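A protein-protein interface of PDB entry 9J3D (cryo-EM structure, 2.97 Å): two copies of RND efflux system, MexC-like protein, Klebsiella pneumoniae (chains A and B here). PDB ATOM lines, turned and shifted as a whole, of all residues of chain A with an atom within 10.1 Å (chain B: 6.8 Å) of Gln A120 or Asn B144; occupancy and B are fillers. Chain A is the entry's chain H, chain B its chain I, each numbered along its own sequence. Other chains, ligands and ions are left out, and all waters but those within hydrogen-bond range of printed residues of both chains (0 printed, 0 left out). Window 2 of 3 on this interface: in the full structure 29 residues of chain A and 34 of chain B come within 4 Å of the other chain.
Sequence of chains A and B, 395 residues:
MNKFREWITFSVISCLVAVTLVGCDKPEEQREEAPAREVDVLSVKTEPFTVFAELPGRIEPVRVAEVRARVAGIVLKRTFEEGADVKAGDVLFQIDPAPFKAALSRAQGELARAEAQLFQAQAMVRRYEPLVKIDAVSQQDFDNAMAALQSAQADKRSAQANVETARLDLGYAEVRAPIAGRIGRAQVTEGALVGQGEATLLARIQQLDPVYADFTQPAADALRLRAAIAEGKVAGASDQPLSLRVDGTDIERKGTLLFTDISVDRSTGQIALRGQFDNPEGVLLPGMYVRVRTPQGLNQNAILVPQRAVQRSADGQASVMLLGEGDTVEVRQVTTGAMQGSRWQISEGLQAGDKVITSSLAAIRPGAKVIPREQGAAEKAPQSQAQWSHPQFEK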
ATOM      1  N   ALA A 112      20.141   0.449   1.937  1.00  0.00           N
ATOM      2  CA  ALA A 112      21.236  -0.167   2.677  1.00  0.00           C
ATOM      3  C   ALA A 112      21.038  -1.671   2.805  1.00  0.00           C
ATOM      4  O   ALA A 112      21.993  -2.446   2.672  1.00  0.00           O
ATOM      5  CB  ALA A 112      21.366   0.477   4.056  1.00  0.00           C
ATOM      6  N   ARG A 113      19.804  -2.102   3.068  1.00  0.00           N
ATOM      7  CA  ARG A 113      19.523  -3.536   3.136  1.00  0.00           C
ATOM      8  C   ARG A 113      19.805  -4.213   1.798  1.00  0.00           C
ATOM      9  O   ARG A 113      20.414  -5.294   1.742  1.00  0.00           O
ATOM     10  CB  ARG A 113      18.073  -3.760   3.563  1.00  0.00           C
ATOM     11  CG  ARG A 113      17.437  -5.012   2.986  1.00  0.00           C
ATOM     12  CD  ARG A 113      15.927  -4.976   3.129  1.00  0.00           C
ATOM     13  NE  ARG A 113      15.476  -5.545   4.393  1.00  0.00           N
ATOM     14  CZ  ARG A 113      15.466  -6.841   4.672  1.00  0.00           C
ATOM     15  NH1 ARG A 113      15.868  -7.741   3.790  1.00  0.00           N
ATOM     16  NH2 ARG A 113      15.043  -7.244   5.865  1.00  0.00           N
ATOM     17  N   ALA A 114      19.369  -3.584   0.705  1.00  0.00           N
ATOM     18  CA  ALA A 114      19.623  -4.146  -0.617  1.00  0.00           C
ATOM     19  C   ALA A 114      21.116  -4.224  -0.905  1.00  0.00           C
ATOM     20  O   ALA A 114      21.594  -5.204  -1.485  1.00  0.00           O
ATOM     21  CB  ALA A 114      18.913  -3.316  -1.686  1.00  0.00           C
ATOM     22  N   GLU A 115      21.867  -3.196  -0.509  1.00  0.00           N
ATOM     23  CA  GLU A 115      23.311  -3.208  -0.717  1.00  0.00           C
ATOM     24  C   GLU A 115      23.976  -4.309   0.096  1.00  0.00           C
ATOM     25  O   GLU A 115      24.933  -4.939  -0.368  1.00  0.00           O
ATOM     26  CB  GLU A 115      23.905  -1.845  -0.365  1.00  0.00           C
ATOM     27  CG  GLU A 115      23.657  -0.774  -1.415  1.00  0.00           C
ATOM     28  CD  GLU A 115      24.379   0.521  -1.107  1.00  0.00           C
ATOM     29  OE1 GLU A 115      24.668   0.774   0.080  1.00  0.00           O
ATOM     30  OE2 GLU A 115      24.661   1.286  -2.053  1.00  0.00           O
ATOM     31  N   ALA A 116      23.492  -4.550   1.315  1.00  0.00           N
ATOM     32  CA  ALA A 116      24.035  -5.643   2.117  1.00  0.00           C
ATOM     33  C   ALA A 116      23.802  -6.988   1.443  1.00  0.00           C
ATOM     34  O   ALA A 116      24.713  -7.828   1.371  1.00  0.00           O
ATOM     35  CB  ALA A 116      23.411  -5.627   3.511  1.00  0.00           C
ATOM     36  N   GLN A 117      22.587  -7.210   0.938  1.00  0.00           N
ATOM     37  CA  GLN A 117      22.314  -8.462   0.236  1.00  0.00           C
ATOM     38  C   GLN A 117      23.174  -8.592  -1.017  1.00  0.00           C
ATOM     39  O   GLN A 117      23.669  -9.684  -1.330  1.00  0.00           O
ATOM     40  CB  GLN A 117      20.830  -8.561  -0.110  1.00  0.00           C
ATOM     41  CG  GLN A 117      19.942  -8.849   1.087  1.00  0.00           C
ATOM     42  CD  GLN A 117      18.469  -8.687   0.771  1.00  0.00           C
ATOM     43  OE1 GLN A 117      18.099  -8.049  -0.214  1.00  0.00           O
ATOM     44  NE2 GLN A 117      17.618  -9.265   1.610  1.00  0.00           N
ATOM     45  N   LEU A 118      23.367  -7.490  -1.744  1.00  0.00           N
ATOM     46  CA  LEU A 118      24.224  -7.527  -2.924  1.00  0.00           C
ATOM     47  C   LEU A 118      25.661  -7.864  -2.552  1.00  0.00           C
ATOM     48  O   LEU A 118      26.336  -8.603  -3.272  1.00  0.00           O
ATOM     49  CB  LEU A 118      24.170  -6.196  -3.669  1.00  0.00           C
ATOM     50  CG  LEU A 118      25.168  -6.116  -4.826  1.00  0.00           C
ATOM     51  CD1 LEU A 118      24.870  -7.190  -5.851  1.00  0.00           C
ATOM     52  CD2 LEU A 118      25.173  -4.750  -5.471  1.00  0.00           C
ATOM     53  N   PHE A 119      26.151  -7.312  -1.441  1.00  0.00           N
ATOM     54  CA  PHE A 119      27.505  -7.629  -0.997  1.00  0.00           C
ATOM     55  C   PHE A 119      27.637  -9.108  -0.666  1.00  0.00           C
ATOM     56  O   PHE A 119      28.639  -9.747  -1.018  1.00  0.00           O
ATOM     57  CB  PHE A 119      27.874  -6.772   0.212  1.00  0.00           C
ATOM     58  CG  PHE A 119      29.202  -7.119   0.817  1.00  0.00           C
ATOM     59  CD1 PHE A 119      30.377  -6.662   0.247  1.00  0.00           C
ATOM     60  CD2 PHE A 119      29.275  -7.896   1.959  1.00  0.00           C
ATOM     61  CE1 PHE A 119      31.601  -6.976   0.802  1.00  0.00           C
ATOM     62  CE2 PHE A 119      30.495  -8.215   2.518  1.00  0.00           C
ATOM     63  CZ  PHE A 119      31.660  -7.754   1.939  1.00  0.00           C
ATOM     64  N   GLN A 120      26.635  -9.670   0.012  1.00  0.00           N
ATOM     65  CA  GLN A 120      26.659 -11.102   0.303  1.00  0.00           C
ATOM     66  C   GLN A 120      26.701 -11.922  -0.980  1.00  0.00           C
ATOM     67  O   GLN A 120      27.485 -12.874  -1.103  1.00  0.00           O
ATOM     68  CB  GLN A 120      25.442 -11.489   1.141  1.00  0.00           C
ATOM     69  CG  GLN A 120      25.394 -12.962   1.498  1.00  0.00           C
ATOM     70  CD  GLN A 120      24.084 -13.362   2.141  1.00  0.00           C
ATOM     71  OE1 GLN A 120      23.225 -12.521   2.400  1.00  0.00           O
ATOM     72  NE2 GLN A 120      23.924 -14.653   2.403  1.00  0.00           N
ATOM     73  N   ALA A 121      25.863 -11.561  -1.953  1.00  0.00           N
ATOM     74  CA  ALA A 121      25.833 -12.301  -3.212  1.00  0.00           C
ATOM     75  C   ALA A 121      27.155 -12.182  -3.959  1.00  0.00           C
ATOM     76  O   ALA A 121      27.638 -13.159  -4.543  1.00  0.00           O
ATOM     77  CB  ALA A 121      24.679 -11.807  -4.080  1.00  0.00           C
ATOM     78  N   GLN A 122      27.750 -10.987  -3.959  1.00  0.00           N
ATOM     79  CA  GLN A 122      29.032 -10.790  -4.627  1.00  0.00           C
ATOM     80  C   GLN A 122      30.120 -11.636  -3.985  1.00  0.00           C
ATOM     81  O   GLN A 122      30.934 -12.246  -4.686  1.00  0.00           O
ATOM     82  CB  GLN A 122      29.423  -9.314  -4.595  1.00  0.00           C
ATOM     83  CG  GLN A 122      28.713  -8.455  -5.620  1.00  0.00           C
ATOM     84  CD  GLN A 122      29.076  -6.992  -5.498  1.00  0.00           C
ATOM     85  OE1 GLN A 122      29.770  -6.589  -4.566  1.00  0.00           O
ATOM     86  NE2 GLN A 122      28.607  -6.185  -6.442  1.00  0.00           N
ATOM     87  N   ALA A 123      30.154 -11.682  -2.651  1.00  0.00           N
ATOM     88  CA  ALA A 123      31.135 -12.527  -1.979  1.00  0.00           C
ATOM     89  C   ALA A 123      30.925 -13.997  -2.313  1.00  0.00           C
ATOM     90  O   ALA A 123      31.898 -14.721  -2.567  1.00  0.00           O
ATOM     91  CB  ALA A 123      31.073 -12.309  -0.468  1.00  0.00           C
ATOM     92  N   MET A 124      29.669 -14.451  -2.331  1.00  0.00           N
ATOM     93  CA  MET A 124      29.391 -15.842  -2.672  1.00  0.00           C
ATOM     94  C   MET A 124      29.865 -16.170  -4.085  1.00  0.00           C
ATOM     95  O   MET A 124      30.492 -17.210  -4.314  1.00  0.00           O
ATOM     96  CB  MET A 124      27.898 -16.128  -2.529  1.00  0.00           C
ATOM     97  CG  MET A 124      27.453 -17.438  -3.152  1.00  0.00           C
ATOM     98  SD  MET A 124      26.089 -18.209  -2.266  1.00  0.00           S
ATOM     99  CE  MET A 124      26.979 -19.158  -1.040  1.00  0.00           C
ATOM    100  N   VAL A 125      29.579 -15.286  -5.042  1.00  0.00           N
ATOM    101  CA  VAL A 125      29.973 -15.538  -6.428  1.00  0.00           C
ATOM    102  C   VAL A 125      31.491 -15.520  -6.560  1.00  0.00           C
ATOM    103  O   VAL A 125      32.080 -16.342  -7.274  1.00  0.00           O
ATOM    104  CB  VAL A 125      29.307 -14.518  -7.368  1.00  0.00           C
ATOM    105  CG1 VAL A 125      29.934 -14.574  -8.749  1.00  0.00           C
ATOM    106  CG2 VAL A 125      27.817 -14.781  -7.450  1.00  0.00           C
ATOM    107  N   ARG A 126      32.147 -14.580  -5.876  1.00  0.00           N
ATOM    108  CA  ARG A 126      33.601 -14.505  -5.936  1.00  0.00           C
ATOM    109  C   ARG A 126      34.247 -15.762  -5.376  1.00  0.00           C
ATOM    110  O   ARG A 126      35.254 -16.232  -5.914  1.00  0.00           O
ATOM    111  CB  ARG A 126      34.096 -13.271  -5.181  1.00  0.00           C
ATOM    112  CG  ARG A 126      33.991 -11.978  -5.973  1.00  0.00           C
ATOM    113  CD  ARG A 126      34.789 -10.861  -5.321  1.00  0.00           C
ATOM    114  NE  ARG A 126      34.373 -10.621  -3.944  1.00  0.00           N
ATOM    115  CZ  ARG A 126      33.967  -9.447  -3.480  1.00  0.00           C
ATOM    116  NH1 ARG A 126      33.904  -8.380  -4.258  1.00  0.00           N
ATOM    117  NH2 ARG A 126      33.612  -9.343  -2.202  1.00  0.00           N
ATOM    118  N   ARG A 127      33.692 -16.315  -4.297  1.00  0.00           N
ATOM    119  CA  ARG A 127      34.236 -17.558  -3.764  1.00  0.00           C
ATOM    120  C   ARG A 127      33.938 -18.745  -4.672  1.00  0.00           C
ATOM    121  O   ARG A 127      34.782 -19.632  -4.828  1.00  0.00           O
ATOM    122  CB  ARG A 127      33.693 -17.819  -2.362  1.00  0.00           C
ATOM    123  CG  ARG A 127      34.476 -17.131  -1.265  1.00  0.00           C
ATOM    124  CD  ARG A 127      33.798 -17.314   0.071  1.00  0.00           C
ATOM    125  NE  ARG A 127      32.788 -16.291   0.299  1.00  0.00           N
ATOM    126  CZ  ARG A 127      32.376 -15.906   1.497  1.00  0.00           C
ATOM    127  NH1 ARG A 127      32.871 -16.438   2.601  1.00  0.00           N
ATOM    128  NH2 ARG A 127      31.443 -14.964   1.589  1.00  0.00           N
ATOM    129  N   TYR A 128      32.746 -18.787  -5.268  1.00  0.00           N
ATOM    130  CA  TYR A 128      32.363 -19.944  -6.071  1.00  0.00           C
ATOM    131  C   TYR A 128      33.046 -19.969  -7.433  1.00  0.00           C
ATOM    132  O   TYR A 128      33.171 -21.044  -8.031  1.00  0.00           O
ATOM    133  CB  TYR A 128      30.846 -19.979  -6.258  1.00  0.00           C
ATOM    134  CG  TYR A 128      30.104 -20.665  -5.137  1.00  0.00           C
ATOM    135  CD1 TYR A 128      30.683 -20.814  -3.887  1.00  0.00           C
ATOM    136  CD2 TYR A 128      28.828 -21.167  -5.330  1.00  0.00           C
ATOM    137  CE1 TYR A 128      30.010 -21.440  -2.859  1.00  0.00           C
ATOM    138  CE2 TYR A 128      28.147 -21.797  -4.309  1.00  0.00           C
ATOM    139  CZ  TYR A 128      28.743 -21.931  -3.076  1.00  0.00           C
ATOM    140  OH  TYR A 128      28.070 -22.557  -2.053  1.00  0.00           O
ATOM    141  N   ASN A 144      22.785 -20.993  -9.414  1.00  0.00           N
ATOM    142  CA  ASN A 144      21.925 -20.411  -8.389  1.00  0.00           C
ATOM    143  C   ASN A 144      22.571 -19.181  -7.766  1.00  0.00           C
ATOM    144  O   ASN A 144      21.903 -18.167  -7.535  1.00  0.00           O
ATOM    145  CB  ASN A 144      21.607 -21.448  -7.313  1.00  0.00           C
ATOM    146  CG  ASN A 144      20.623 -22.496  -7.785  1.00  0.00           C
ATOM    147  OD1 ASN A 144      19.927 -22.307  -8.780  1.00  0.00           O
ATOM    148  ND2 ASN A 144      20.560 -23.611  -7.070  1.00  0.00           N
ATOM    149  N   ALA A 145      23.874 -19.253  -7.490  1.00  0.00           N
ATOM    150  CA  ALA A 145      24.577 -18.102  -6.934  1.00  0.00           C
ATOM    151  C   ALA A 145      24.579 -16.931  -7.908  1.00  0.00           C
ATOM    152  O   ALA A 145      24.399 -15.777  -7.500  1.00  0.00           O
ATOM    153  CB  ALA A 145      26.006 -18.489  -6.559  1.00  0.00           C
ATOM    154  N   MET A 146      24.785 -17.205  -9.197  1.00  0.00           N
ATOM    155  CA  MET A 146      24.766 -16.133 -10.188  1.00  0.00           C
ATOM    156  C   MET A 146      23.382 -15.504 -10.296  1.00  0.00           C
ATOM    157  O   MET A 146      23.252 -14.280 -10.422  1.00  0.00           O
ATOM    158  CB  MET A 146      25.225 -16.661 -11.547  1.00  0.00           C
ATOM    159  CG  MET A 146      26.736 -16.704 -11.734  1.00  0.00           C
ATOM    160  SD  MET A 146      27.578 -15.128 -12.021  1.00  0.00           S
ATOM    161  CE  MET A 146      26.232 -14.025 -12.455  1.00  0.00           C
ATOM    162  N   ALA A 148      21.175 -15.373  -7.893  1.00  0.00           N
ATOM    163  CA  ALA A 148      21.014 -14.570  -6.687  1.00  0.00           C
ATOM    164  C   ALA A 148      21.755 -13.246  -6.807  1.00  0.00           C
ATOM    165  O   ALA A 148      21.255 -12.205  -6.368  1.00  0.00           O
ATOM    166  CB  ALA A 148      21.499 -15.349  -5.467  1.00  0.00           C
ATOM    167  N   LEU A 149      22.952 -13.265  -7.394  1.00  0.00           N
ATOM    168  CA  LEU A 149      23.709 -12.031  -7.583  1.00  0.00           C
ATOM    169  C   LEU A 149      22.967 -11.067  -8.500  1.00  0.00           C
ATOM    170  O   LEU A 149      22.885  -9.863  -8.224  1.00  0.00           O
ATOM    171  CB  LEU A 149      25.091 -12.351  -8.147  1.00  0.00           C
ATOM    172  CG  LEU A 149      25.903 -11.167  -8.667  1.00  0.00           C
ATOM    173  CD1 LEU A 149      26.187 -10.185  -7.550  1.00  0.00           C
ATOM    174  CD2 LEU A 149      27.194 -11.640  -9.312  1.00  0.00           C
ATOM    175  N   GLN A 150      22.425 -11.580  -9.604  1.00  0.00           N
ATOM    176  CA  GLN A 150      21.684 -10.724 -10.526  1.00  0.00           C
ATOM    177  C   GLN A 150      20.420 -10.174  -9.872  1.00  0.00           C
ATOM    178  O   GLN A 150      20.074  -8.999 -10.055  1.00  0.00           O
ATOM    179  CB  GLN A 150      21.352 -11.497 -11.799  1.00  0.00           C
ATOM    180  CG  GLN A 150      22.576 -11.843 -12.632  1.00  0.00           C
ATOM    181  CD  GLN A 150      22.262 -12.774 -13.785  1.00  0.00           C
ATOM    182  OE1 GLN A 150      21.137 -13.249 -13.926  1.00  0.00           O
ATOM    183  NE2 GLN A 150      23.260 -13.041 -14.618  1.00  0.00           N
ATOM    184  N   ALA A 152      20.038  -9.614  -6.680  1.00  0.00           N
ATOM    185  CA  ALA A 152      20.481  -8.595  -5.737  1.00  0.00           C
ATOM    186  C   ALA A 152      20.830  -7.292  -6.441  1.00  0.00           C
ATOM    187  O   ALA A 152      20.527  -6.211  -5.926  1.00  0.00           O
ATOM    188  CB  ALA A 152      21.676  -9.105  -4.938  1.00  0.00           C
ATOM    189  N   GLN A 153      21.475  -7.371  -7.607  1.00  0.00           N
ATOM    190  CA  GLN A 153      21.753  -6.157  -8.371  1.00  0.00           C
ATOM    191  C   GLN A 153      20.461  -5.456  -8.772  1.00  0.00           C
ATOM    192  O   GLN A 153      20.347  -4.227  -8.661  1.00  0.00           O
ATOM    193  CB  GLN A 153      22.584  -6.492  -9.609  1.00  0.00           C
ATOM    194  CG  GLN A 153      24.028  -6.848  -9.315  1.00  0.00           C
ATOM    195  CD  GLN A 153      24.768  -7.343 -10.541  1.00  0.00           C
ATOM    196  OE1 GLN A 153      24.171  -7.561 -11.593  1.00  0.00           O
ATOM    197  NE2 GLN A 153      26.076  -7.525 -10.408  1.00  0.00           N
ATOM    198  N   VAL B 125      26.278 -12.655  15.478  1.00  0.00           N
ATOM    199  CA  VAL B 125      27.551 -12.157  14.961  1.00  0.00           C
ATOM    200  C   VAL B 125      28.616 -12.178  16.052  1.00  0.00           C
ATOM    201  O   VAL B 125      29.773 -12.544  15.811  1.00  0.00           O
ATOM    202  CB  VAL B 125      27.376 -10.749  14.367  1.00  0.00           C
ATOM    203  CG1 VAL B 125      28.726 -10.114  14.095  1.00  0.00           C
ATOM    204  CG2 VAL B 125      26.558 -10.819  13.093  1.00  0.00           C
ATOM    205  N   SER B 138      32.560 -21.724   8.920  1.00  0.00           N
ATOM    206  CA  SER B 138      32.953 -21.345   7.573  1.00  0.00           C
ATOM    207  C   SER B 138      32.898 -19.832   7.403  1.00  0.00           C
ATOM    208  O   SER B 138      32.101 -19.141   8.042  1.00  0.00           O
ATOM    209  CB  SER B 138      32.048 -22.015   6.543  1.00  0.00           C
ATOM    210  OG  SER B 138      30.815 -21.327   6.428  1.00  0.00           O
ATOM    211  N   GLN B 139      33.768 -19.320   6.531  1.00  0.00           N
ATOM    212  CA  GLN B 139      33.736 -17.898   6.210  1.00  0.00           C
ATOM    213  C   GLN B 139      32.396 -17.510   5.598  1.00  0.00           C
ATOM    214  O   GLN B 139      31.905 -16.394   5.809  1.00  0.00           O
ATOM    215  CB  GLN B 139      34.884 -17.553   5.262  1.00  0.00           C
ATOM    216  CG  GLN B 139      35.074 -16.068   5.004  1.00  0.00           C
ATOM    217  CD  GLN B 139      35.576 -15.321   6.221  1.00  0.00           C
ATOM    218  OE1 GLN B 139      36.382 -15.841   6.992  1.00  0.00           O
ATOM    219  NE2 GLN B 139      35.103 -14.094   6.399  1.00  0.00           N
ATOM    220  N   GLN B 140      31.789 -18.424   4.840  1.00  0.00           N
ATOM    221  CA  GLN B 140      30.492 -18.147   4.234  1.00  0.00           C
ATOM    222  C   GLN B 140      29.417 -17.955   5.295  1.00  0.00           C
ATOM    223  O   GLN B 140      28.565 -17.068   5.170  1.00  0.00           O
ATOM    224  CB  GLN B 140      30.110 -19.276   3.281  1.00  0.00           C
ATOM    225  CG  GLN B 140      28.796 -19.057   2.565  1.00  0.00           C
ATOM    226  CD  GLN B 140      28.803 -17.801   1.722  1.00  0.00           C
ATOM    227  OE1 GLN B 140      29.766 -17.526   1.006  1.00  0.00           O
ATOM    228  NE2 GLN B 140      27.727 -17.028   1.804  1.00  0.00           N
ATOM    229  N   ASP B 141      29.435 -18.779   6.343  1.00  0.00           N
ATOM    230  CA  ASP B 141      28.458 -18.625   7.418  1.00  0.00           C
ATOM    231  C   ASP B 141      28.637 -17.296   8.140  1.00  0.00           C
ATOM    232  O   ASP B 141      27.652 -16.627   8.475  1.00  0.00           O
ATOM    233  CB  ASP B 141      28.570 -19.789   8.400  1.00  0.00           C
ATOM    234  CG  ASP B 141      28.064 -21.091   7.817  1.00  0.00           C
ATOM    235  OD1 ASP B 141      26.986 -21.083   7.186  1.00  0.00           O
ATOM    236  OD2 ASP B 141      28.743 -22.125   7.990  1.00  0.00           O
ATOM    237  N   PHE B 142      29.884 -16.897   8.391  1.00  0.00           N
ATOM    238  CA  PHE B 142      30.134 -15.617   9.045  1.00  0.00           C
ATOM    239  C   PHE B 142      29.670 -14.459   8.172  1.00  0.00           C
ATOM    240  O   PHE B 142      29.103 -13.479   8.670  1.00  0.00           O
ATOM    241  CB  PHE B 142      31.617 -15.481   9.382  1.00  0.00           C
ATOM    242  CG  PHE B 142      31.976 -14.166  10.007  1.00  0.00           C
ATOM    243  CD1 PHE B 142      31.592 -13.873  11.302  1.00  0.00           C
ATOM    244  CD2 PHE B 142      32.698 -13.224   9.300  1.00  0.00           C
ATOM    245  CE1 PHE B 142      31.921 -12.666  11.879  1.00  0.00           C
ATOM    246  CE2 PHE B 142      33.030 -12.014   9.873  1.00  0.00           C
ATOM    247  CZ  PHE B 142      32.641 -11.735  11.164  1.00  0.00           C
ATOM    248  N   ASP B 143      29.908 -14.549   6.862  1.00  0.00           N
ATOM    249  CA  ASP B 143      29.440 -13.502   5.960  1.00  0.00           C
ATOM    250  C   ASP B 143      27.919 -13.447   5.917  1.00  0.00           C
ATOM    251  O   ASP B 143      27.331 -12.362   5.859  1.00  0.00           O
ATOM    252  CB  ASP B 143      30.015 -13.711   4.562  1.00  0.00           C
ATOM    253  CG  ASP B 143      31.492 -13.383   4.491  1.00  0.00           C
ATOM    254  OD1 ASP B 143      32.015 -12.789   5.454  1.00  0.00           O
ATOM    255  OD2 ASP B 143      32.129 -13.709   3.470  1.00  0.00           O
ATOM    256  N   ASN B 144      27.262 -14.608   5.942  1.00  0.00           N
ATOM    257  CA  ASN B 144      25.805 -14.627   6.001  1.00  0.00           C
ATOM    258  C   ASN B 144      25.303 -13.975   7.281  1.00  0.00           C
ATOM    259  O   ASN B 144      24.329 -13.213   7.260  1.00  0.00           O
ATOM    260  CB  ASN B 144      25.295 -16.064   5.897  1.00  0.00           C
ATOM    261  CG  ASN B 144      25.490 -16.651   4.518  1.00  0.00           C
ATOM    262  OD1 ASN B 144      25.685 -15.925   3.545  1.00  0.00           O
ATOM    263  ND2 ASN B 144      25.439 -17.972   4.424  1.00  0.00           N
ATOM    264  N   ALA B 145      25.957 -14.262   8.407  1.00  0.00           N
ATOM    265  CA  ALA B 145      25.565 -13.645   9.669  1.00  0.00           C
ATOM    266  C   ALA B 145      25.756 -12.134   9.630  1.00  0.00           C
ATOM    267  O   ALA B 145      24.910 -11.382  10.128  1.00  0.00           O
ATOM    268  CB  ALA B 145      26.360 -14.256  10.820  1.00  0.00           C
ATOM    269  N   MET B 146      26.862 -11.671   9.047  1.00  0.00           N
ATOM    270  CA  MET B 146      27.097 -10.233   8.953  1.00  0.00           C
ATOM    271  C   MET B 146      26.072  -9.564   8.046  1.00  0.00           C
ATOM    272  O   MET B 146      25.605  -8.454   8.334  1.00  0.00           O
ATOM    273  CB  MET B 146      28.516  -9.961   8.452  1.00  0.00           C
ATOM    274  CG  MET B 146      29.576  -9.892   9.549  1.00  0.00           C
ATOM    275  SD  MET B 146      29.412  -8.573  10.777  1.00  0.00           S
ATOM    276  CE  MET B 146      28.546  -7.288   9.875  1.00  0.00           C
ATOM    277  N   ALA B 147      25.716 -10.218   6.939  1.00  0.00           N
ATOM    278  CA  ALA B 147      24.678  -9.682   6.066  1.00  0.00           C
ATOM    279  C   ALA B 147      23.342  -9.610   6.789  1.00  0.00           C
ATOM    280  O   ALA B 147      22.595  -8.638   6.637  1.00  0.00           O
ATOM    281  CB  ALA B 147      24.561 -10.531   4.802  1.00  0.00           C
ATOM    282  N   ALA B 148      23.025 -10.634   7.585  1.00  0.00           N
ATOM    283  CA  ALA B 148      21.799 -10.601   8.375  1.00  0.00           C
ATOM    284  C   ALA B 148      21.825  -9.461   9.385  1.00  0.00           C
ATOM    285  O   ALA B 148      20.806  -8.800   9.609  1.00  0.00           O
ATOM    286  CB  ALA B 148      21.595 -11.940   9.081  1.00  0.00           C
ATOM    287  N   LEU B 149      22.980  -9.219  10.008  1.00  0.00           N
ATOM    288  CA  LEU B 149      23.096  -8.117  10.959  1.00  0.00           C
ATOM    289  C   LEU B 149      22.881  -6.772  10.275  1.00  0.00           C
ATOM    290  O   LEU B 149      22.186  -5.895  10.802  1.00  0.00           O
ATOM    291  CB  LEU B 149      24.461  -8.159  11.643  1.00  0.00           C
ATOM    292  CG  LEU B 149      24.851  -6.933  12.468  1.00  0.00           C
ATOM    293  CD1 LEU B 149      23.850  -6.702  13.578  1.00  0.00           C
ATOM    294  CD2 LEU B 149      26.249  -7.087  13.034  1.00  0.00           C
ATOM    295  N   GLN B 150      23.486  -6.586   9.100  1.00  0.00           N
ATOM    296  CA  GLN B 150      23.297  -5.337   8.367  1.00  0.00           C
ATOM    297  C   GLN B 150      21.841  -5.161   7.952  1.00  0.00           C
ATOM    298  O   GLN B 150      21.288  -4.055   8.035  1.00  0.00           O
ATOM    299  CB  GLN B 150      24.218  -5.302   7.148  1.00  0.00           C
ATOM    300  CG  GLN B 150      25.693  -5.197   7.499  1.00  0.00           C
ATOM    301  CD  GLN B 150      26.595  -5.254   6.282  1.00  0.00           C
ATOM    302  OE1 GLN B 150      26.131  -5.439   5.160  1.00  0.00           O
ATOM    303  NE2 GLN B 150      27.895  -5.096   6.500  1.00  0.00           N
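Ala A116 touches Gln B150 (CB to OE1, 3.2 Å).
Gln A120 touches Ala B147 (OE1 to CB, 3.4 Å).
Met A124 touches Gln B140 (CE to CD, 3.6 Å).
Of the 14 printed residues of chain B, 6 touch a printed residue of chain A.
Printed residues of chain B that touch a printed residue of chain A: Gln B139, Gln B140, Asp B143, Asn B144, Ala B147 and Gln B150.
Along chain B the printed residues that touch a printed residue of chain A span positions 139 to 150.
Of the 25 printed residues of chain A, 4 touch a printed residue of chain B.
Hydrophobic or aromatic side chains of chain A within 4 Å of the printed part of chain B: Ala A116 and Met A124.
Among the printed residues, 7 pairs touch across the chains.
Among the printed residues, Asp or Glu carboxylates within 4 Å of a Lys or Arg side-chain nitrogen of the other chain: Arg A127 with Asp B143 (2.4 Å).
The backbone carbonyl oxygen (O) of Ala A123 sits at hydrogen-bond distance from the guanidinium group (NE) of Arg A127 (3.4 Å).
The side-chain hydroxyl (OG) of Ser B138 sits close to the backbone NH (N) of Gln B140, at 3.4 Å.
The side-chain carboxylate (OD1) of Asp B143 is in hydrogen-bond range of the side-chain amide nitrogen (NE2) of Gln B139 (3.5 Å).
OD1 of Asn B144 lies within hydrogen-bond range of NE2 of Gln B140, 2.9 Å away.
7 positions are printed for both chains.
Of the 7 pairs that touch across the chains among the printed residues, none has its exchanged pair printed and touching as well.
The side-chain amide nitrogen (NE2) of Gln A120 sits at hydrogen-bond distance from the side-chain amide oxygen (OD1) of Asn B144.
The guanidinium group of Arg A127 lies close to the backbone carbonyl oxygen of Gln B139 (3.4 Å).
The guanidinium group (NH2) of Arg A127 sits close to the side-chain amide oxygen (OE1) of Gln B140 (3.1 Å).
OD2 of Asp B143 lies within salt-bridge range of NH1 of Arg A127 (3.0 Å).
Of the printed residues of chain B, Ala A116 touches Gln B150 (3.2 Å).
Gln A120 touches two residues of chain B.
Printed residues of chain B within 4 Å of Met A124: Gln B140 (3.6 Å).
Met A146 touches none of the printed residues of chain B.
Of the printed residues of chain A, Gln B139 touches Arg A127.
Gln B140 touches two residues of chain A.
Asp B143 touches just one residue of chain A: Arg A127 (2.4 Å).
Of chain A, only Gln A120 (2.5 Å) comes within 4 Å of Asn B144.
Ala B145 touches none of the printed residues of chain A.
Of chain A, only Gln A120 comes within 4 Å of Ala B147.
Of the printed residues of chain A, Gln B150 touches Ala A116 (3.2 Å).
The nearest residue of chain B that does not touch Gln A120 is Gln B140 (4.5 Å).
The nearest residue of chain A that does not touch Asn B144 is Met A124 (5.8 Å).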
